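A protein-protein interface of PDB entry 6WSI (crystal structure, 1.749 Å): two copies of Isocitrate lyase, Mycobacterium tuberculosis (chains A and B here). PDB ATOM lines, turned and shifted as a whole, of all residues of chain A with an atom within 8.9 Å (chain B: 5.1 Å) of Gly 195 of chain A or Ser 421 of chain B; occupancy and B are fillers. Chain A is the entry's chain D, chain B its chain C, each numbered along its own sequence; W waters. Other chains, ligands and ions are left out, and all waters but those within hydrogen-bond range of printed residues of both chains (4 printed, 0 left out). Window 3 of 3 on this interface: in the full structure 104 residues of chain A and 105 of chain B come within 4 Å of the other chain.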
ATOM      1  N   ASP A 108      -1.753   5.426 -13.680  1.00  0.00           N
ATOM      2  CA  ASP A 108      -0.670   6.413 -13.748  1.00  0.00           C
ATOM      3  C   ASP A 108      -0.757   7.389 -12.574  1.00  0.00           C
ATOM      4  O   ASP A 108      -1.127   8.554 -12.723  1.00  0.00           O
ATOM      5  CB  ASP A 108      -0.738   7.144 -15.080  1.00  0.00           C
ATOM      6  CG  ASP A 108       0.478   8.005 -15.331  1.00  0.00           C
ATOM      7  OD1 ASP A 108       1.508   7.784 -14.663  1.00  0.00           O
ATOM      8  OD2 ASP A 108       0.387   8.908 -16.182  1.00  0.00           O
ATOM      9  N   GLN A 109      -0.374   6.889 -11.383  1.00  0.00           N
ATOM     10  CA  GLN A 109      -0.561   7.620 -10.131  1.00  0.00           C
ATOM     11  C   GLN A 109       0.664   7.535  -9.216  1.00  0.00           C
ATOM     12  O   GLN A 109       0.532   7.617  -7.989  1.00  0.00           O
ATOM     13  CB  GLN A 109      -1.822   7.123  -9.406  1.00  0.00           C
ATOM     14  CG  GLN A 109      -3.076   7.310 -10.271  1.00  0.00           C
ATOM     15  CD  GLN A 109      -4.386   6.926  -9.581  1.00  0.00           C
ATOM     16  OE1 GLN A 109      -5.073   6.019 -10.031  1.00  0.00           O
ATOM     17  NE2 GLN A 109      -4.736   7.627  -8.509  1.00  0.00           N
ATOM     18  N   GLN A 184       2.906  18.680 -10.221  1.00  0.00           N
ATOM     19  CA  GLN A 184       1.849  18.033  -9.451  1.00  0.00           C
ATOM     20  C   GLN A 184       2.335  17.626  -8.060  1.00  0.00           C
ATOM     21  O   GLN A 184       3.534  17.453  -7.810  1.00  0.00           O
ATOM     22  CB  GLN A 184       1.338  16.788 -10.175  1.00  0.00           C
ATOM     23  CG  GLN A 184       0.645  17.043 -11.504  1.00  0.00           C
ATOM     24  CD  GLN A 184      -0.015  15.771 -12.030  1.00  0.00           C
ATOM     25  OE1 GLN A 184      -0.733  15.098 -11.293  1.00  0.00           O
ATOM     26  NE2 GLN A 184       0.253  15.424 -13.294  1.00  0.00           N
ATOM     27  N   GLU A 188      -0.490  12.711  -4.949  1.00  0.00           N
ATOM     28  CA  GLU A 188      -1.762  12.666  -5.663  1.00  0.00           C
ATOM     29  C   GLU A 188      -1.551  12.711  -7.172  1.00  0.00           C
ATOM     30  O   GLU A 188      -2.445  13.123  -7.920  1.00  0.00           O
ATOM     31  CB  GLU A 188      -2.679  13.801  -5.207  1.00  0.00           C
ATOM     32  CG  GLU A 188      -3.052  13.733  -3.718  1.00  0.00           C
ATOM     33  CD  GLU A 188      -3.963  12.556  -3.375  1.00  0.00           C
ATOM     34  OE1 GLU A 188      -4.675  12.059  -4.278  1.00  0.00           O
ATOM     35  OE2 GLU A 188      -3.966  12.128  -2.193  1.00  0.00           O
ATOM     36  N   LYS A 189      -0.382  12.263  -7.630  1.00  0.00           N
ATOM     37  CA  LYS A 189      -0.018  12.394  -9.037  1.00  0.00           C
ATOM     38  C   LYS A 189      -1.024  11.678  -9.935  1.00  0.00           C
ATOM     39  O   LYS A 189      -1.510  10.589  -9.612  1.00  0.00           O
ATOM     40  CB  LYS A 189       1.390  11.831  -9.263  1.00  0.00           C
ATOM     41  CG  LYS A 189       1.943  11.962 -10.694  1.00  0.00           C
ATOM     42  CD  LYS A 189       1.582  10.729 -11.539  1.00  0.00           C
ATOM     43  CE  LYS A 189       2.363  10.689 -12.853  1.00  0.00           C
ATOM     44  NZ  LYS A 189       2.007  11.773 -13.807  1.00  0.00           N
ATOM     45  N   LYS A 190      -1.320  12.292 -11.081  1.00  0.00           N
ATOM     46  CA  LYS A 190      -2.188  11.711 -12.093  1.00  0.00           C
ATOM     47  C   LYS A 190      -1.540  11.853 -13.462  1.00  0.00           C
ATOM     48  O   LYS A 190      -0.761  12.779 -13.710  1.00  0.00           O
ATOM     49  CB  LYS A 190      -3.577  12.393 -12.134  1.00  0.00           C
ATOM     50  CG  LYS A 190      -4.290  12.457 -10.809  1.00  0.00           C
ATOM     51  CD  LYS A 190      -4.873  11.101 -10.464  1.00  0.00           C
ATOM     52  CE  LYS A 190      -5.892  11.184  -9.331  1.00  0.00           C
ATOM     53  NZ  LYS A 190      -5.316  11.734  -8.081  1.00  0.00           N
ATOM     54  N   CYS A 191      -1.883  10.933 -14.363  1.00  0.00           N
ATOM     55  CA  CYS A 191      -1.744  11.214 -15.788  1.00  0.00           C
ATOM     56  C   CYS A 191      -2.396  12.559 -16.094  1.00  0.00           C
ATOM     57  O   CYS A 191      -3.426  12.912 -15.503  1.00  0.00           O
ATOM     58  CB  CYS A 191      -2.395  10.093 -16.605  1.00  0.00           C
ATOM     59  SG  CYS A 191      -2.715  10.428 -18.367  1.00  0.00           S
ATOM     60  N   GLY A 192      -1.775  13.324 -16.997  1.00  0.00           N
ATOM     61  CA  GLY A 192      -2.283  14.652 -17.303  1.00  0.00           C
ATOM     62  C   GLY A 192      -3.709  14.659 -17.807  1.00  0.00           C
ATOM     63  O   GLY A 192      -4.373  15.704 -17.753  1.00  0.00           O
ATOM     64  N   HIS A 193      -4.204  13.513 -18.280  1.00  0.00           N
ATOM     65  CA  HIS A 193      -5.538  13.420 -18.851  1.00  0.00           C
ATOM     66  C   HIS A 193      -6.500  12.634 -17.971  1.00  0.00           C
ATOM     67  O   HIS A 193      -7.584  12.254 -18.431  1.00  0.00           O
ATOM     68  CB  HIS A 193      -5.434  12.842 -20.261  1.00  0.00           C
ATOM     69  CG  HIS A 193      -4.531  13.648 -21.141  1.00  0.00           C
ATOM     70  ND1 HIS A 193      -3.313  13.184 -21.589  1.00  0.00           N
ATOM     71  CD2 HIS A 193      -4.638  14.923 -21.591  1.00  0.00           C
ATOM     72  CE1 HIS A 193      -2.729  14.120 -22.317  1.00  0.00           C
ATOM     73  NE2 HIS A 193      -3.507  15.189 -22.326  1.00  0.00           N
ATOM     74  N   LEU A 194      -6.131  12.399 -16.714  1.00  0.00           N
ATOM     75  CA  LEU A 194      -7.039  11.938 -15.675  1.00  0.00           C
ATOM     76  C   LEU A 194      -7.497  13.137 -14.848  1.00  0.00           C
ATOM     77  O   LEU A 194      -6.897  14.218 -14.891  1.00  0.00           O
ATOM     78  CB  LEU A 194      -6.354  10.893 -14.780  1.00  0.00           C
ATOM     79  CG  LEU A 194      -6.168   9.494 -15.377  1.00  0.00           C
ATOM     80  CD1 LEU A 194      -5.201   8.634 -14.525  1.00  0.00           C
ATOM     81  CD2 LEU A 194      -7.526   8.812 -15.545  1.00  0.00           C
ATOM     82  N   GLY A 195      -8.572  12.933 -14.078  1.00  0.00           N
ATOM     83  CA  GLY A 195      -9.036  13.933 -13.141  1.00  0.00           C
ATOM     84  C   GLY A 195      -8.350  13.811 -11.787  1.00  0.00           C
ATOM     85  O   GLY A 195      -7.513  12.938 -11.554  1.00  0.00           O
ATOM     86  N   GLY A 196      -8.726  14.713 -10.880  1.00  0.00           N
ATOM     87  CA  GLY A 196      -8.181  14.681  -9.533  1.00  0.00           C
ATOM     88  C   GLY A 196      -6.764  15.199  -9.399  1.00  0.00           C
ATOM     89  O   GLY A 196      -6.036  14.765  -8.494  1.00  0.00           O
ATOM     90  N   LYS A 197      -6.348  16.125 -10.262  1.00  0.00           N
ATOM     91  CA  LYS A 197      -4.980  16.631 -10.249  1.00  0.00           C
ATOM     92  C   LYS A 197      -4.841  17.759  -9.235  1.00  0.00           C
ATOM     93  O   LYS A 197      -5.733  18.597  -9.092  1.00  0.00           O
ATOM     94  CB  LYS A 197      -4.565  17.122 -11.637  1.00  0.00           C
ATOM     95  CG  LYS A 197      -4.685  16.062 -12.725  1.00  0.00           C
ATOM     96  CD  LYS A 197      -3.771  16.351 -13.908  1.00  0.00           C
ATOM     97  CE  LYS A 197      -4.110  17.672 -14.577  1.00  0.00           C
ATOM     98  NZ  LYS A 197      -3.478  17.761 -15.927  1.00  0.00           N
ATOM     99  N   VAL A 198      -3.708  17.782  -8.543  1.00  0.00           N
ATOM    100  CA  VAL A 198      -3.393  18.812  -7.559  1.00  0.00           C
ATOM    101  C   VAL A 198      -2.057  19.441  -7.936  1.00  0.00           C
ATOM    102  O   VAL A 198      -1.043  18.738  -8.003  1.00  0.00           O
ATOM    103  CB  VAL A 198      -3.329  18.236  -6.139  1.00  0.00           C
ATOM    104  CG1 VAL A 198      -3.101  19.357  -5.122  1.00  0.00           C
ATOM    105  CG2 VAL A 198      -4.611  17.450  -5.822  1.00  0.00           C
ATOM    106  N   ALA A 233      -5.776  21.843 -16.815  1.00  0.00           N
ATOM    107  CA  ALA A 233      -6.947  21.126 -16.323  1.00  0.00           C
ATOM    108  C   ALA A 233      -7.060  21.066 -14.805  1.00  0.00           C
ATOM    109  O   ALA A 233      -8.173  20.891 -14.298  1.00  0.00           O
ATOM    110  CB  ALA A 233      -6.967  19.688 -16.870  1.00  0.00           C
ATOM    111  N   ALA A 234      -5.960  21.197 -14.066  1.00  0.00           N
ATOM    112  CA  ALA A 234      -6.030  21.058 -12.613  1.00  0.00           C
ATOM    113  C   ALA A 234      -6.867  22.181 -11.995  1.00  0.00           C
ATOM    114  O   ALA A 234      -6.670  23.357 -12.311  1.00  0.00           O
ATOM    115  CB  ALA A 234      -4.623  21.067 -12.012  1.00  0.00           C
ATOM    116  N   THR A 235      -7.792  21.825 -11.096  1.00  0.00           N
ATOM    117  CA  THR A 235      -8.568  22.820 -10.360  1.00  0.00           C
ATOM    118  C   THR A 235      -8.207  22.865  -8.879  1.00  0.00           C
ATOM    119  O   THR A 235      -8.938  23.473  -8.092  1.00  0.00           O
ATOM    120  CB  THR A 235     -10.076  22.568 -10.510  1.00  0.00           C
ATOM    121  OG1 THR A 235     -10.409  21.293  -9.957  1.00  0.00           O
ATOM    122  CG2 THR A 235     -10.486  22.595 -11.975  1.00  0.00           C
ATOM    123  N   LEU A 236      -7.104  22.237  -8.479  1.00  0.00           N
ATOM    124  CA  LEU A 236      -6.678  22.202  -7.086  1.00  0.00           C
ATOM    125  C   LEU A 236      -5.193  22.550  -6.997  1.00  0.00           C
ATOM    126  O   LEU A 236      -4.414  22.240  -7.904  1.00  0.00           O
ATOM    127  CB  LEU A 236      -6.931  20.825  -6.464  1.00  0.00           C
ATOM    128  CG  LEU A 236      -8.389  20.351  -6.348  1.00  0.00           C
ATOM    129  CD1 LEU A 236      -8.447  18.910  -5.864  1.00  0.00           C
ATOM    130  CD2 LEU A 236      -9.145  21.263  -5.399  1.00  0.00           C
ATOM    131  N   GLY A 287      -6.037  19.369 -23.103  1.00  0.00           N
ATOM    132  CA  GLY A 287      -7.192  18.487 -23.088  1.00  0.00           C
ATOM    133  C   GLY A 287      -7.623  17.979 -24.453  1.00  0.00           C
ATOM    134  O   GLY A 287      -8.401  17.025 -24.539  1.00  0.00           O
ATOM    135  N   SER A 317      -4.536   9.577 -25.406  1.00  0.00           N
ATOM    136  CA  SER A 317      -5.724   9.867 -24.608  1.00  0.00           C
ATOM    137  C   SER A 317      -6.700  10.781 -25.340  1.00  0.00           C
ATOM    138  O   SER A 317      -7.810  11.008 -24.842  1.00  0.00           O
ATOM    139  CB  SER A 317      -5.315  10.489 -23.274  1.00  0.00           C
ATOM    140  OG  SER A 317      -4.606   9.552 -22.464  1.00  0.00           O
ATOM    141  N   THR B 415      -9.877  13.646  -4.971  1.00  0.00           N
ATOM    142  CA  THR B 415      -8.758  13.408  -5.878  1.00  0.00           C
ATOM    143  C   THR B 415      -8.836  12.035  -6.543  1.00  0.00           C
ATOM    144  O   THR B 415      -7.807  11.396  -6.789  1.00  0.00           O
ATOM    145  CB  THR B 415      -7.425  13.571  -5.152  1.00  0.00           C
ATOM    146  OG1 THR B 415      -7.344  12.645  -4.060  1.00  0.00           O
ATOM    147  CG2 THR B 415      -7.282  14.983  -4.616  1.00  0.00           C
ATOM    148  N   THR B 416     -10.045  11.567  -6.875  1.00  0.00           N
ATOM    149  CA  THR B 416     -10.178  10.347  -7.667  1.00  0.00           C
ATOM    150  C   THR B 416      -9.897  10.638  -9.151  1.00  0.00           C
ATOM    151  O   THR B 416      -9.890  11.792  -9.597  1.00  0.00           O
ATOM    152  CB  THR B 416     -11.567   9.716  -7.474  1.00  0.00           C
ATOM    153  OG1 THR B 416     -12.593  10.630  -7.878  1.00  0.00           O
ATOM    154  CG2 THR B 416     -11.784   9.342  -6.008  1.00  0.00           C
ATOM    155  N   ALA B 417      -9.663   9.570  -9.924  1.00  0.00           N
ATOM    156  CA  ALA B 417      -8.997   9.674 -11.226  1.00  0.00           C
ATOM    157  C   ALA B 417      -9.941   9.717 -12.427  1.00  0.00           C
ATOM    158  O   ALA B 417      -9.765  10.560 -13.318  1.00  0.00           O
ATOM    159  CB  ALA B 417      -8.012   8.513 -11.409  1.00  0.00           C
ATOM    160  N   LEU B 418     -10.924   8.812 -12.505  1.00  0.00           N
ATOM    161  CA  LEU B 418     -11.672   8.693 -13.757  1.00  0.00           C
ATOM    162  C   LEU B 418     -12.624   9.871 -13.981  1.00  0.00           C
ATOM    163  O   LEU B 418     -12.833  10.283 -15.130  1.00  0.00           O
ATOM    164  CB  LEU B 418     -12.426   7.361 -13.802  1.00  0.00           C
ATOM    165  CG  LEU B 418     -11.607   6.175 -14.344  1.00  0.00           C
ATOM    166  CD1 LEU B 418     -12.460   4.919 -14.408  1.00  0.00           C
ATOM    167  CD2 LEU B 418     -11.000   6.482 -15.716  1.00  0.00           C
ATOM    168  N   THR B 419     -13.194  10.429 -12.912  1.00  0.00           N
ATOM    169  CA  THR B 419     -14.088  11.579 -13.038  1.00  0.00           C
ATOM    170  C   THR B 419     -13.314  12.782 -13.571  1.00  0.00           C
ATOM    171  O   THR B 419     -12.341  13.220 -12.951  1.00  0.00           O
ATOM    172  CB  THR B 419     -14.725  11.907 -11.687  1.00  0.00           C
ATOM    173  OG1 THR B 419     -15.569  10.825 -11.269  1.00  0.00           O
ATOM    174  CG2 THR B 419     -15.553  13.183 -11.776  1.00  0.00           C
ATOM    175  N   GLY B 420     -13.744  13.321 -14.717  1.00  0.00           N
ATOM    176  CA  GLY B 420     -13.069  14.448 -15.329  1.00  0.00           C
ATOM    177  C   GLY B 420     -11.926  14.093 -16.259  1.00  0.00           C
ATOM    178  O   GLY B 420     -11.253  15.004 -16.767  1.00  0.00           O
ATOM    179  N   SER B 421     -11.682  12.806 -16.495  1.00  0.00           N
ATOM    180  CA  SER B 421     -10.640  12.362 -17.410  1.00  0.00           C
ATOM    181  C   SER B 421     -11.077  12.568 -18.860  1.00  0.00           C
ATOM    182  O   SER B 421     -12.269  12.648 -19.167  1.00  0.00           O
ATOM    183  CB  SER B 421     -10.324  10.886 -17.165  1.00  0.00           C
ATOM    184  OG  SER B 421     -11.518  10.110 -17.202  1.00  0.00           O
ATOM    185  N   THR B 422     -10.089  12.644 -19.766  1.00  0.00           N
ATOM    186  CA  THR B 422     -10.421  12.662 -21.189  1.00  0.00           C
ATOM    187  C   THR B 422     -10.961  11.320 -21.665  1.00  0.00           C
ATOM    188  O   THR B 422     -11.676  11.280 -22.672  1.00  0.00           O
ATOM    189  CB  THR B 422      -9.208  13.043 -22.049  1.00  0.00           C
ATOM    190  OG1 THR B 422      -8.177  12.056 -21.898  1.00  0.00           O
ATOM    191  CG2 THR B 422      -8.673  14.425 -21.667  1.00  0.00           C
ATOM    192  N   GLU B 423     -10.628  10.219 -20.979  1.00  0.00           N
ATOM    193  CA  GLU B 423     -11.245   8.939 -21.315  1.00  0.00           C
ATOM    194  C   GLU B 423     -12.753   8.979 -21.073  1.00  0.00           C
ATOM    195  O   GLU B 423     -13.536   8.499 -21.903  1.00  0.00           O
ATOM    196  CB  GLU B 423     -10.593   7.815 -20.509  1.00  0.00           C
ATOM    197  CG  GLU B 423     -11.258   6.444 -20.676  1.00  0.00           C
ATOM    198  CD  GLU B 423     -10.325   5.311 -20.267  1.00  0.00           C
ATOM    199  OE1 GLU B 423      -9.259   5.165 -20.898  1.00  0.00           O
ATOM    200  OE2 GLU B 423     -10.652   4.596 -19.314  1.00  0.00           O
ATOM    201  N   GLU B 424     -13.176   9.568 -19.952  1.00  0.00           N
ATOM    202  CA  GLU B 424     -14.602   9.711 -19.670  1.00  0.00           C
ATOM    203  C   GLU B 424     -15.269  10.703 -20.624  1.00  0.00           C
ATOM    204  O   GLU B 424     -16.444  10.535 -20.975  1.00  0.00           O
ATOM    205  CB  GLU B 424     -14.790  10.131 -18.207  1.00  0.00           C
ATOM    206  CG  GLU B 424     -16.179  10.610 -17.815  1.00  0.00           C
ATOM    207  CD  GLU B 424     -16.229  11.107 -16.372  1.00  0.00           C
ATOM    208  OE1 GLU B 424     -16.468  10.281 -15.460  1.00  0.00           O
ATOM    209  OE2 GLU B 424     -16.003  12.319 -16.151  1.00  0.00           O
ATOM    210  N   GLY B 425     -14.537  11.717 -21.076  1.00  0.00           N
ATOM    211  CA  GLY B 425     -15.122  12.736 -21.925  1.00  0.00           C
ATOM    212  C   GLY B 425     -15.058  12.483 -23.419  1.00  0.00           C
ATOM    213  O   GLY B 425     -15.828  13.088 -24.173  1.00  0.00           O
HETATM  214  O   HOH W   1      -7.729   9.685 -20.272  1.00  0.00           O
HETATM  215  O   HOH W   2      -7.136   8.479  -6.270  1.00  0.00           O
HETATM  216  O   HOH W   3      -8.262   8.954 -22.506  1.00  0.00           O
HETATM  217  O   HOH W   4     -11.792  13.564 -10.047  1.00  0.00           O
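NZ of Lys 190 of chain A sits at hydrogen-bond distance from O of Thr 415 of chain B, 2.8 Å away. The side-chain hydroxyl (OG1) of Thr 422 of chain B lies within hydrogen-bond range of the backbone carbonyl oxygen (O) of Ser 317 of chain A (3.1 Å). The backbone carbonyl oxygen of Ala 417 of chain B lies within hydrogen-bond range of the backbone NH of Gly 195 of chain A, 2.8 Å away. The backbone carbonyl oxygen of Thr 416 of chain B sits close to the backbone carbonyl oxygen of Gly 195 of chain A (3.3 Å). The backbone carbonyl oxygen (O) of Thr 416 of chain B sits close to the backbone NH (N) of Gly 196 of chain A, 3.4 Å away. OE1 of Glu 188 of chain A lies within hydrogen-bond range of OG1 of Thr 415 of chain B. O of His 193 of chain A sits at hydrogen-bond distance from N of Thr 422 of chain B (2.9 Å).
SG of Cys 191 of chain A sits close to N of His 193 of chain A (3.4 Å). The backbone carbonyl oxygen of Lys 190 of chain A lies within hydrogen-bond range of the side-chain amide nitrogen of Gln 184 of chain A (2.9 Å). O of Gly 196 of chain A lies within hydrogen-bond range of NZ of Lys 190 of chain A (3.1 Å). The side-chain carboxylate of Glu 188 of chain A is in salt-bridge range of the side-chain amino group of Lys 190 of chain A. The side-chain hydroxyl (OG) of Ser 421 of chain B is in hydrogen-bond range of the backbone NH (N) of Glu 424 of chain B, 3.3 Å away. The side-chain hydroxyl (OG) of Ser 421 of chain B lies within hydrogen-bond range of the backbone carbonyl oxygen (O) of Leu 418 of chain B (2.5 Å).
Among the printed residues, merely in contact across the chains: His 193 of chain A with Ser 421 of chain B, Gly 195 of chain A with Thr 419 of chain B, Leu 194 of chain A with Ala 417 of chain B, Leu 194 of chain A with Ser 421 of chain B, Gly 196 of chain A with Thr 415 of chain B, Val 198 of chain A with Thr 415 of chain B, Gly 287 of chain A with Thr 422 of chain B, Lys 190 of chain A with Ala 417 of chain B and Gly 195 of chain A with Ser 421 of chain B.
Of the printed residues of chain B, Lys 190 of chain A touches Thr 415 and Ala 417. Of chain B, only Thr 416, Ala 417, Thr 419 and Ser 421 come within 4 Å of Gly 195 of chain A. Of the printed residues of chain B, Gly 196 of chain A touches Thr 415 (3.8 Å) and Thr 416 (3.4 Å). Printed residues of chain B within 4 Å of Gly 287 of chain A: Thr 422. Printed residues of chain A within 4 Å of Thr 415 of chain B: Glu 188 (2.7 Å), Lys 190 (2.8 Å), Gly 196 (3.8 Å) and Val 198 (3.8 Å). Ala 417 of chain B touches just these residues of chain A: Lys 190 (3.9 Å), Leu 194 (3.6 Å) and Gly 195 (2.8 Å). Of the printed residues of chain A, Thr 419 of chain B touches Gly 195 (3.4 Å). Ser 421 of chain B touches just these residues of chain A: His 193 (3.2 Å), Leu 194 (3.8 Å) and Gly 195 (3.9 Å). Of the printed residues of chain A, Thr 422 of chain B touches His 193 (2.9 Å), Gly 287 (3.9 Å) and Ser 317 (3.1 Å). The nearest residue of chain B that does not touch Gly 195 of chain A is Gly 420 of chain B (4.2 Å). The nearest residue of chain A that does not touch Ser 421 of chain B is Gly 196 of chain A (6.6 Å).
Hydrophobic or aromatic side chains of chain B that line the printed part of chain A: Ala 417. Hydrophobic or aromatic side chains of chain A that line the printed part of chain B: His 193, Leu 194 and Val 198. Among the printed residues, 16 pairs touch across the chains. Among the printed residues, no Asp or Glu carboxylate lies within 4 Å of a Lys or Arg side-chain nitrogen of the other chain.
No position is printed for both chains. Of the 16 pairs that touch across the chains among the printed residues, none has its exchanged pair printed and touching as well.
Water W4 lies within hydrogen-bond range of the backbone carbonyl oxygen (O) of Thr 416 of chain B (2.6 Å), the backbone carbonyl oxygen (O) of Thr 419 of chain B (3.0 Å) and the backbone NH (N) of Gly 196 of chain A (3.4 Å). Water W1 lies within hydrogen-bond range of the side-chain hydroxyl (OG1) of Thr 422 of chain B (2.9 Å), the backbone NH (N) of Glu 423 of chain B (3.0 Å) and the backbone carbonyl oxygen (O) of His 193 of chain A (3.2 Å). Water W2 lies within hydrogen-bond range of O of Thr 415 of chain B and NE2 of Gln 109 of chain A. Water W3 lies within hydrogen-bond range of N of Glu 423 of chain B (3.1 Å), O of Ser 317 of chain A (3.1 Å) and OG1 of Thr 422 of chain B (3.2 Å).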
